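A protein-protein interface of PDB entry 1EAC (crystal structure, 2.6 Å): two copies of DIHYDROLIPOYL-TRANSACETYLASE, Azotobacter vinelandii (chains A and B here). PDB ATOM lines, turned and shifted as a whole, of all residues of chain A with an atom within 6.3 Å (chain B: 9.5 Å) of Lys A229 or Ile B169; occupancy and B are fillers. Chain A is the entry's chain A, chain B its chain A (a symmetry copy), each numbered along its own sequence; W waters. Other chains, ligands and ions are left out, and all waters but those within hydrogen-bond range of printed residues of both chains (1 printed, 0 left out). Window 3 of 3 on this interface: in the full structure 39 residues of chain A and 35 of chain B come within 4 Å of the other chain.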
ATOM      1  N   GLU A  45     -22.284  -6.392 -21.544  1.00  0.00           N
ATOM      2  CA  GLU A  45     -23.600  -6.987 -21.745  1.00  0.00           C
ATOM      3  C   GLU A  45     -24.652  -6.102 -21.048  1.00  0.00           C
ATOM      4  O   GLU A  45     -24.213  -5.317 -20.197  1.00  0.00           O
ATOM      5  CB  GLU A  45     -23.635  -8.386 -21.146  1.00  0.00           C
ATOM      6  CG  GLU A  45     -24.959  -9.096 -21.299  1.00  0.00           C
ATOM      7  CD  GLU A  45     -25.373  -9.348 -22.747  1.00  0.00           C
ATOM      8  OE1 GLU A  45     -25.894  -8.468 -23.447  1.00  0.00           O
ATOM      9  OE2 GLU A  45     -25.146 -10.455 -23.205  1.00  0.00           O
ATOM     10  N   GLY A 221     -12.641 -15.994 -24.759  1.00  0.00           N
ATOM     11  CA  GLY A 221     -13.696 -15.083 -25.102  1.00  0.00           C
ATOM     12  C   GLY A 221     -15.044 -15.735 -25.098  1.00  0.00           C
ATOM     13  O   GLY A 221     -16.004 -15.198 -24.555  1.00  0.00           O
ATOM     14  N   ALA A 222     -15.204 -16.933 -25.633  1.00  0.00           N
ATOM     15  CA  ALA A 222     -16.540 -17.514 -25.575  1.00  0.00           C
ATOM     16  C   ALA A 222     -16.960 -17.887 -24.178  1.00  0.00           C
ATOM     17  O   ALA A 222     -18.134 -17.750 -23.896  1.00  0.00           O
ATOM     18  CB  ALA A 222     -16.655 -18.750 -26.360  1.00  0.00           C
ATOM     19  N   ALA A 223     -16.112 -18.267 -23.228  1.00  0.00           N
ATOM     20  CA  ALA A 223     -16.597 -18.621 -21.908  1.00  0.00           C
ATOM     21  C   ALA A 223     -17.125 -17.394 -21.216  1.00  0.00           C
ATOM     22  O   ALA A 223     -18.118 -17.452 -20.492  1.00  0.00           O
ATOM     23  CB  ALA A 223     -15.497 -19.161 -21.093  1.00  0.00           C
ATOM     24  N   ALA A 224     -16.518 -16.244 -21.489  1.00  0.00           N
ATOM     25  CA  ALA A 224     -16.944 -15.021 -20.848  1.00  0.00           C
ATOM     26  C   ALA A 224     -18.155 -14.420 -21.486  1.00  0.00           C
ATOM     27  O   ALA A 224     -18.890 -13.778 -20.751  1.00  0.00           O
ATOM     28  CB  ALA A 224     -15.881 -13.983 -20.892  1.00  0.00           C
ATOM     29  N   ALA A 225     -18.409 -14.587 -22.796  1.00  0.00           N
ATOM     30  CA  ALA A 225     -19.623 -14.054 -23.406  1.00  0.00           C
ATOM     31  C   ALA A 225     -20.786 -14.861 -22.923  1.00  0.00           C
ATOM     32  O   ALA A 225     -21.874 -14.317 -22.813  1.00  0.00           O
ATOM     33  CB  ALA A 225     -19.653 -14.155 -24.891  1.00  0.00           C
ATOM     34  N   ARG A 226     -20.552 -16.149 -22.629  1.00  0.00           N
ATOM     35  CA  ARG A 226     -21.508 -17.074 -22.025  1.00  0.00           C
ATOM     36  C   ARG A 226     -21.721 -16.728 -20.553  1.00  0.00           C
ATOM     37  O   ARG A 226     -22.850 -16.814 -20.065  1.00  0.00           O
ATOM     38  CB  ARG A 226     -20.956 -18.436 -22.151  1.00  0.00           C
ATOM     39  CG  ARG A 226     -21.914 -19.575 -21.855  1.00  0.00           C
ATOM     40  CD  ARG A 226     -21.100 -20.893 -21.963  1.00  0.00           C
ATOM     41  NE  ARG A 226     -20.247 -21.050 -23.162  1.00  0.00           N
ATOM     42  CZ  ARG A 226     -20.747 -21.239 -24.411  1.00  0.00           C
ATOM     43  NH1 ARG A 226     -22.075 -21.307 -24.701  1.00  0.00           N
ATOM     44  NH2 ARG A 226     -19.893 -21.354 -25.439  1.00  0.00           N
ATOM     45  N   PHE A 227     -20.726 -16.327 -19.769  1.00  0.00           N
ATOM     46  CA  PHE A 227     -20.988 -15.890 -18.419  1.00  0.00           C
ATOM     47  C   PHE A 227     -21.876 -14.665 -18.434  1.00  0.00           C
ATOM     48  O   PHE A 227     -22.866 -14.680 -17.711  1.00  0.00           O
ATOM     49  CB  PHE A 227     -19.710 -15.538 -17.732  1.00  0.00           C
ATOM     50  CG  PHE A 227     -19.827 -15.205 -16.258  1.00  0.00           C
ATOM     51  CD1 PHE A 227     -20.164 -13.927 -15.847  1.00  0.00           C
ATOM     52  CD2 PHE A 227     -19.546 -16.191 -15.341  1.00  0.00           C
ATOM     53  CE1 PHE A 227     -20.231 -13.622 -14.503  1.00  0.00           C
ATOM     54  CE2 PHE A 227     -19.608 -15.884 -13.995  1.00  0.00           C
ATOM     55  CZ  PHE A 227     -19.947 -14.601 -13.580  1.00  0.00           C
ATOM     56  N   THR A 228     -21.635 -13.598 -19.198  1.00  0.00           N
ATOM     57  CA  THR A 228     -22.472 -12.412 -19.120  1.00  0.00           C
ATOM     58  C   THR A 228     -23.865 -12.709 -19.625  1.00  0.00           C
ATOM     59  O   THR A 228     -24.857 -12.182 -19.134  1.00  0.00           O
ATOM     60  CB  THR A 228     -21.888 -11.232 -19.935  1.00  0.00           C
ATOM     61  OG1 THR A 228     -21.586 -11.728 -21.233  1.00  0.00           O
ATOM     62  CG2 THR A 228     -20.702 -10.591 -19.276  1.00  0.00           C
ATOM     63  N   LYS A 229     -23.976 -13.594 -20.611  1.00  0.00           N
ATOM     64  CA  LYS A 229     -25.262 -14.019 -21.141  1.00  0.00           C
ATOM     65  C   LYS A 229     -26.075 -14.740 -20.068  1.00  0.00           C
ATOM     66  O   LYS A 229     -27.223 -14.347 -19.853  1.00  0.00           O
ATOM     67  CB  LYS A 229     -25.027 -14.949 -22.319  1.00  0.00           C
ATOM     68  CG  LYS A 229     -26.164 -14.901 -23.268  1.00  0.00           C
ATOM     69  CD  LYS A 229     -26.973 -16.196 -23.294  1.00  0.00           C
ATOM     70  CE  LYS A 229     -28.181 -15.983 -24.275  1.00  0.00           C
ATOM     71  NZ  LYS A 229     -27.796 -15.495 -25.627  1.00  0.00           N
ATOM     72  N   ARG A 230     -25.524 -15.757 -19.386  1.00  0.00           N
ATOM     73  CA  ARG A 230     -26.237 -16.433 -18.343  1.00  0.00           C
ATOM     74  C   ARG A 230     -26.589 -15.448 -17.281  1.00  0.00           C
ATOM     75  O   ARG A 230     -27.722 -15.457 -16.854  1.00  0.00           O
ATOM     76  CB  ARG A 230     -25.401 -17.505 -17.736  1.00  0.00           C
ATOM     77  CG  ARG A 230     -25.302 -18.762 -18.562  1.00  0.00           C
ATOM     78  CD  ARG A 230     -26.697 -19.319 -18.461  1.00  0.00           C
ATOM     79  NE  ARG A 230     -27.049 -19.900 -17.168  1.00  0.00           N
ATOM     80  CZ  ARG A 230     -28.313 -19.953 -16.719  1.00  0.00           C
ATOM     81  NH1 ARG A 230     -29.367 -19.454 -17.383  1.00  0.00           N
ATOM     82  NH2 ARG A 230     -28.574 -20.638 -15.614  1.00  0.00           N
ATOM     83  N   LEU A 231     -25.721 -14.547 -16.849  1.00  0.00           N
ATOM     84  CA  LEU A 231     -26.068 -13.578 -15.824  1.00  0.00           C
ATOM     85  C   LEU A 231     -27.221 -12.674 -16.255  1.00  0.00           C
ATOM     86  O   LEU A 231     -28.146 -12.389 -15.482  1.00  0.00           O
ATOM     87  CB  LEU A 231     -24.824 -12.762 -15.497  1.00  0.00           C
ATOM     88  CG  LEU A 231     -24.911 -11.757 -14.371  1.00  0.00           C
ATOM     89  CD1 LEU A 231     -25.352 -12.492 -13.133  1.00  0.00           C
ATOM     90  CD2 LEU A 231     -23.581 -11.047 -14.175  1.00  0.00           C
ATOM     91  N   GLY A 232     -27.239 -12.230 -17.497  1.00  0.00           N
ATOM     92  CA  GLY A 232     -28.313 -11.405 -17.991  1.00  0.00           C
ATOM     93  C   GLY A 232     -29.618 -12.174 -17.936  1.00  0.00           C
ATOM     94  O   GLY A 232     -30.652 -11.610 -17.582  1.00  0.00           O
ATOM     95  N   ASP A 233     -29.575 -13.472 -18.266  1.00  0.00           N
ATOM     96  CA  ASP A 233     -30.724 -14.363 -18.193  1.00  0.00           C
ATOM     97  C   ASP A 233     -31.186 -14.555 -16.767  1.00  0.00           C
ATOM     98  O   ASP A 233     -32.384 -14.614 -16.545  1.00  0.00           O
ATOM     99  CB  ASP A 233     -30.446 -15.756 -18.662  1.00  0.00           C
ATOM    100  CG  ASP A 233     -30.264 -16.063 -20.133  1.00  0.00           C
ATOM    101  OD1 ASP A 233     -30.679 -15.272 -20.992  1.00  0.00           O
ATOM    102  OD2 ASP A 233     -29.714 -17.145 -20.395  1.00  0.00           O
ATOM    103  N   LEU A 234     -30.292 -14.736 -15.799  1.00  0.00           N
ATOM    104  CA  LEU A 234     -30.667 -14.927 -14.427  1.00  0.00           C
ATOM    105  C   LEU A 234     -31.276 -13.678 -13.861  1.00  0.00           C
ATOM    106  O   LEU A 234     -32.310 -13.732 -13.239  1.00  0.00           O
ATOM    107  CB  LEU A 234     -29.457 -15.295 -13.628  1.00  0.00           C
ATOM    108  CG  LEU A 234     -28.975 -16.709 -13.750  1.00  0.00           C
ATOM    109  CD1 LEU A 234     -27.910 -16.884 -12.730  1.00  0.00           C
ATOM    110  CD2 LEU A 234     -30.054 -17.723 -13.408  1.00  0.00           C
ATOM    111  N   ALA B 112     -10.865 -16.633 -35.032  1.00  0.00           N
ATOM    112  CA  ALA B 112     -10.683 -17.373 -33.813  1.00  0.00           C
ATOM    113  C   ALA B 112     -11.613 -18.538 -33.624  1.00  0.00           C
ATOM    114  O   ALA B 112     -12.821 -18.313 -33.698  1.00  0.00           O
ATOM    115  CB  ALA B 112     -10.832 -16.385 -32.667  1.00  0.00           C
ATOM    116  N   ASP B 114     -12.948 -21.297 -30.824  1.00  0.00           N
ATOM    117  CA  ASP B 114     -12.647 -21.769 -29.477  1.00  0.00           C
ATOM    118  C   ASP B 114     -12.964 -23.267 -29.450  1.00  0.00           C
ATOM    119  O   ASP B 114     -14.086 -23.681 -29.777  1.00  0.00           O
ATOM    120  CB  ASP B 114     -13.474 -21.011 -28.395  1.00  0.00           C
ATOM    121  CG  ASP B 114     -13.064 -19.530 -28.081  1.00  0.00           C
ATOM    122  OD1 ASP B 114     -11.965 -19.249 -27.562  1.00  0.00           O
ATOM    123  OD2 ASP B 114     -13.864 -18.607 -28.334  1.00  0.00           O
ATOM    124  N   SER B 165     -15.222 -13.482 -33.567  1.00  0.00           N
ATOM    125  CA  SER B 165     -16.647 -13.273 -33.515  1.00  0.00           C
ATOM    126  C   SER B 165     -17.294 -14.000 -32.367  1.00  0.00           C
ATOM    127  O   SER B 165     -17.209 -15.225 -32.236  1.00  0.00           O
ATOM    128  CB  SER B 165     -17.231 -13.740 -34.846  1.00  0.00           C
ATOM    129  OG  SER B 165     -18.651 -13.658 -34.881  1.00  0.00           O
ATOM    130  N   LEU B 166     -17.996 -13.300 -31.493  1.00  0.00           N
ATOM    131  CA  LEU B 166     -18.737 -13.961 -30.432  1.00  0.00           C
ATOM    132  C   LEU B 166     -20.209 -13.721 -30.656  1.00  0.00           C
ATOM    133  O   LEU B 166     -20.993 -14.112 -29.811  1.00  0.00           O
ATOM    134  CB  LEU B 166     -18.261 -13.404 -29.100  1.00  0.00           C
ATOM    135  CG  LEU B 166     -16.769 -13.592 -28.819  1.00  0.00           C
ATOM    136  CD1 LEU B 166     -16.366 -13.012 -27.487  1.00  0.00           C
ATOM    137  CD2 LEU B 166     -16.487 -15.066 -28.745  1.00  0.00           C
ATOM    138  N   GLY B 167     -20.611 -13.143 -31.784  1.00  0.00           N
ATOM    139  CA  GLY B 167     -21.995 -12.862 -32.060  1.00  0.00           C
ATOM    140  C   GLY B 167     -22.917 -14.057 -31.822  1.00  0.00           C
ATOM    141  O   GLY B 167     -24.041 -13.932 -31.344  1.00  0.00           O
ATOM    142  N   HIS B 168     -22.455 -15.257 -32.142  1.00  0.00           N
ATOM    143  CA  HIS B 168     -23.209 -16.469 -31.891  1.00  0.00           C
ATOM    144  C   HIS B 168     -23.471 -16.769 -30.419  1.00  0.00           C
ATOM    145  O   HIS B 168     -24.156 -17.741 -30.110  1.00  0.00           O
ATOM    146  CB  HIS B 168     -22.458 -17.630 -32.516  1.00  0.00           C
ATOM    147  CG  HIS B 168     -21.096 -17.916 -31.927  1.00  0.00           C
ATOM    148  ND1 HIS B 168     -20.681 -19.004 -31.291  1.00  0.00           N
ATOM    149  CD2 HIS B 168     -20.025 -17.067 -31.930  1.00  0.00           C
ATOM    150  CE1 HIS B 168     -19.420 -18.860 -30.934  1.00  0.00           C
ATOM    151  NE2 HIS B 168     -19.030 -17.672 -31.333  1.00  0.00           N
ATOM    152  N   ILE B 169     -22.892 -16.051 -29.440  1.00  0.00           N
ATOM    153  CA  ILE B 169     -23.109 -16.314 -28.033  1.00  0.00           C
ATOM    154  C   ILE B 169     -23.716 -15.062 -27.444  1.00  0.00           C
ATOM    155  O   ILE B 169     -24.744 -15.196 -26.796  1.00  0.00           O
ATOM    156  CB  ILE B 169     -21.807 -16.625 -27.351  1.00  0.00           C
ATOM    157  CG1 ILE B 169     -21.294 -17.889 -27.910  1.00  0.00           C
ATOM    158  CG2 ILE B 169     -21.998 -16.800 -25.874  1.00  0.00           C
ATOM    159  CD1 ILE B 169     -19.882 -18.096 -27.450  1.00  0.00           C
ATOM    160  N   GLY B 170     -23.205 -13.845 -27.574  1.00  0.00           N
ATOM    161  CA  GLY B 170     -23.930 -12.772 -26.957  1.00  0.00           C
ATOM    162  C   GLY B 170     -23.037 -11.629 -26.609  1.00  0.00           C
ATOM    163  O   GLY B 170     -21.890 -11.556 -27.062  1.00  0.00           O
ATOM    164  N   GLY B 171     -23.582 -10.688 -25.854  1.00  0.00           N
ATOM    165  CA  GLY B 171     -22.775  -9.558 -25.499  1.00  0.00           C
ATOM    166  C   GLY B 171     -22.957  -8.430 -26.475  1.00  0.00           C
ATOM    167  O   GLY B 171     -23.396  -8.523 -27.607  1.00  0.00           O
ATOM    168  N   THR B 172     -22.483  -7.341 -25.975  1.00  0.00           N
ATOM    169  CA  THR B 172     -22.630  -6.038 -26.566  1.00  0.00           C
ATOM    170  C   THR B 172     -21.355  -5.496 -27.177  1.00  0.00           C
ATOM    171  O   THR B 172     -21.433  -4.668 -28.071  1.00  0.00           O
ATOM    172  CB  THR B 172     -23.214  -5.295 -25.356  1.00  0.00           C
ATOM    173  OG1 THR B 172     -24.605  -5.373 -25.649  1.00  0.00           O
ATOM    174  CG2 THR B 172     -22.726  -3.929 -25.047  1.00  0.00           C
ATOM    175  N   VAL B 188     -16.568  -9.057 -32.980  1.00  0.00           N
ATOM    176  CA  VAL B 188     -17.913  -8.893 -33.498  1.00  0.00           C
ATOM    177  C   VAL B 188     -18.819  -9.474 -32.458  1.00  0.00           C
ATOM    178  O   VAL B 188     -18.681 -10.653 -32.097  1.00  0.00           O
ATOM    179  CB  VAL B 188     -18.134  -9.664 -34.813  1.00  0.00           C
ATOM    180  CG1 VAL B 188     -19.545  -9.395 -35.299  1.00  0.00           C
ATOM    181  CG2 VAL B 188     -17.197  -9.195 -35.890  1.00  0.00           C
ATOM    182  N   SER B 189     -19.744  -8.679 -31.960  1.00  0.00           N
ATOM    183  CA  SER B 189     -20.636  -9.212 -30.949  1.00  0.00           C
ATOM    184  C   SER B 189     -21.991  -9.393 -31.539  1.00  0.00           C
ATOM    185  O   SER B 189     -22.110  -9.355 -32.749  1.00  0.00           O
ATOM    186  CB  SER B 189     -20.731  -8.287 -29.768  1.00  0.00           C
ATOM    187  OG  SER B 189     -19.470  -8.077 -29.169  1.00  0.00           O
ATOM    188  N   LYS B 190     -23.040  -9.484 -30.754  1.00  0.00           N
ATOM    189  CA  LYS B 190     -24.321  -9.909 -31.226  1.00  0.00           C
ATOM    190  C   LYS B 190     -25.159  -8.822 -31.839  1.00  0.00           C
ATOM    191  O   LYS B 190     -25.209  -7.750 -31.252  1.00  0.00           O
ATOM    192  CB  LYS B 190     -24.982 -10.522 -30.043  1.00  0.00           C
ATOM    193  CG  LYS B 190     -26.221 -11.282 -30.401  1.00  0.00           C
ATOM    194  CD  LYS B 190     -27.021 -11.304 -29.126  1.00  0.00           C
ATOM    195  CE  LYS B 190     -28.407 -11.912 -29.373  1.00  0.00           C
ATOM    196  NZ  LYS B 190     -28.357 -13.371 -29.469  1.00  0.00           N
ATOM    197  N   ALA B 191     -25.824  -9.044 -32.983  1.00  0.00           N
ATOM    198  CA  ALA B 191     -26.636  -8.033 -33.636  1.00  0.00           C
ATOM    199  C   ALA B 191     -27.963  -7.985 -32.943  1.00  0.00           C
ATOM    200  O   ALA B 191     -28.489  -9.029 -32.514  1.00  0.00           O
ATOM    201  CB  ALA B 191     -26.912  -8.366 -35.051  1.00  0.00           C
HETATM  202  O   HOH W   1     -26.584 -11.234 -25.371  1.00  0.00           O
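O of Ala A225 is in hydrogen-bond range of OG1 of Thr A228, at 3.0 Å. N of Lys B190 sits at hydrogen-bond distance from O of Gly B171 (3.3 Å). O of Val B188 lies within hydrogen-bond range of N of Leu B166.
Lys A229 touches just one residue of chain B: Ile B169 (3.3 Å). Of chain B, only Asp B114 (3.4 Å), Leu B166 (3.8 Å) and Ile B169 (3.5 Å) come within 4 Å of Ala A222. No residue of chain B comes within 4 Å of Thr A228. No residue of chain B comes within 4 Å of Gly A232. Of the printed residues of chain B, Glu A45 touches Gly B171. Of the printed residues of chain A, Asp B114 touches Ala A222 (3.4 Å). Printed residues of chain B within 4 Å of Arg A226: Ile B169. Of the printed residues of chain A, Gly B171 touches Glu A45. Of the printed residues of chain B, Gly A221 touches Leu B166. Ala B112 touches none of the printed residues of chain A. Arg A230 touches none of the printed residues of chain B. The nearest printed residue of chain B that does not touch Glu A45 is Thr B172 (4.01 Å).
No position is printed for both chains.
Of the 15 printed residues of chain A, 6 touch a printed residue of chain B. Printed residues of chain A that touch a printed residue of chain B: Glu A45, Gly A221, Ala A222, Ala A225, Arg A226 and Lys A229. Among the printed residues, 8 pairs touch across the chains.
O of Ile B169 lies within hydrogen-bond range of NZ of Lys A229 (3.3 Å). The side-chain carboxylate (OE2) of Glu A45 lies within hydrogen-bond range of the backbone NH (N) of Gly B171 (3.1 Å). The backbone NH (N) of Ala A222 sits close to the side-chain carboxylate (OD2) of Asp B114 (3.4 Å).
Gly A221 touches Leu B166. N of Ala A222 touches CD2 of Leu B166, 3.8 Å away. Ala A222 touches Ile B169 (CB to CD1, 3.5 Å). CB of Ala A225 touches CG2 of Ile B169, 3.7 Å away. Ile B169 touches Arg A226.
Water W1 bridges the side-chain carboxylate (OE2) of Glu A45 (2.7 Å) and the backbone NH (N) of Gly B171 (3.1 Å).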
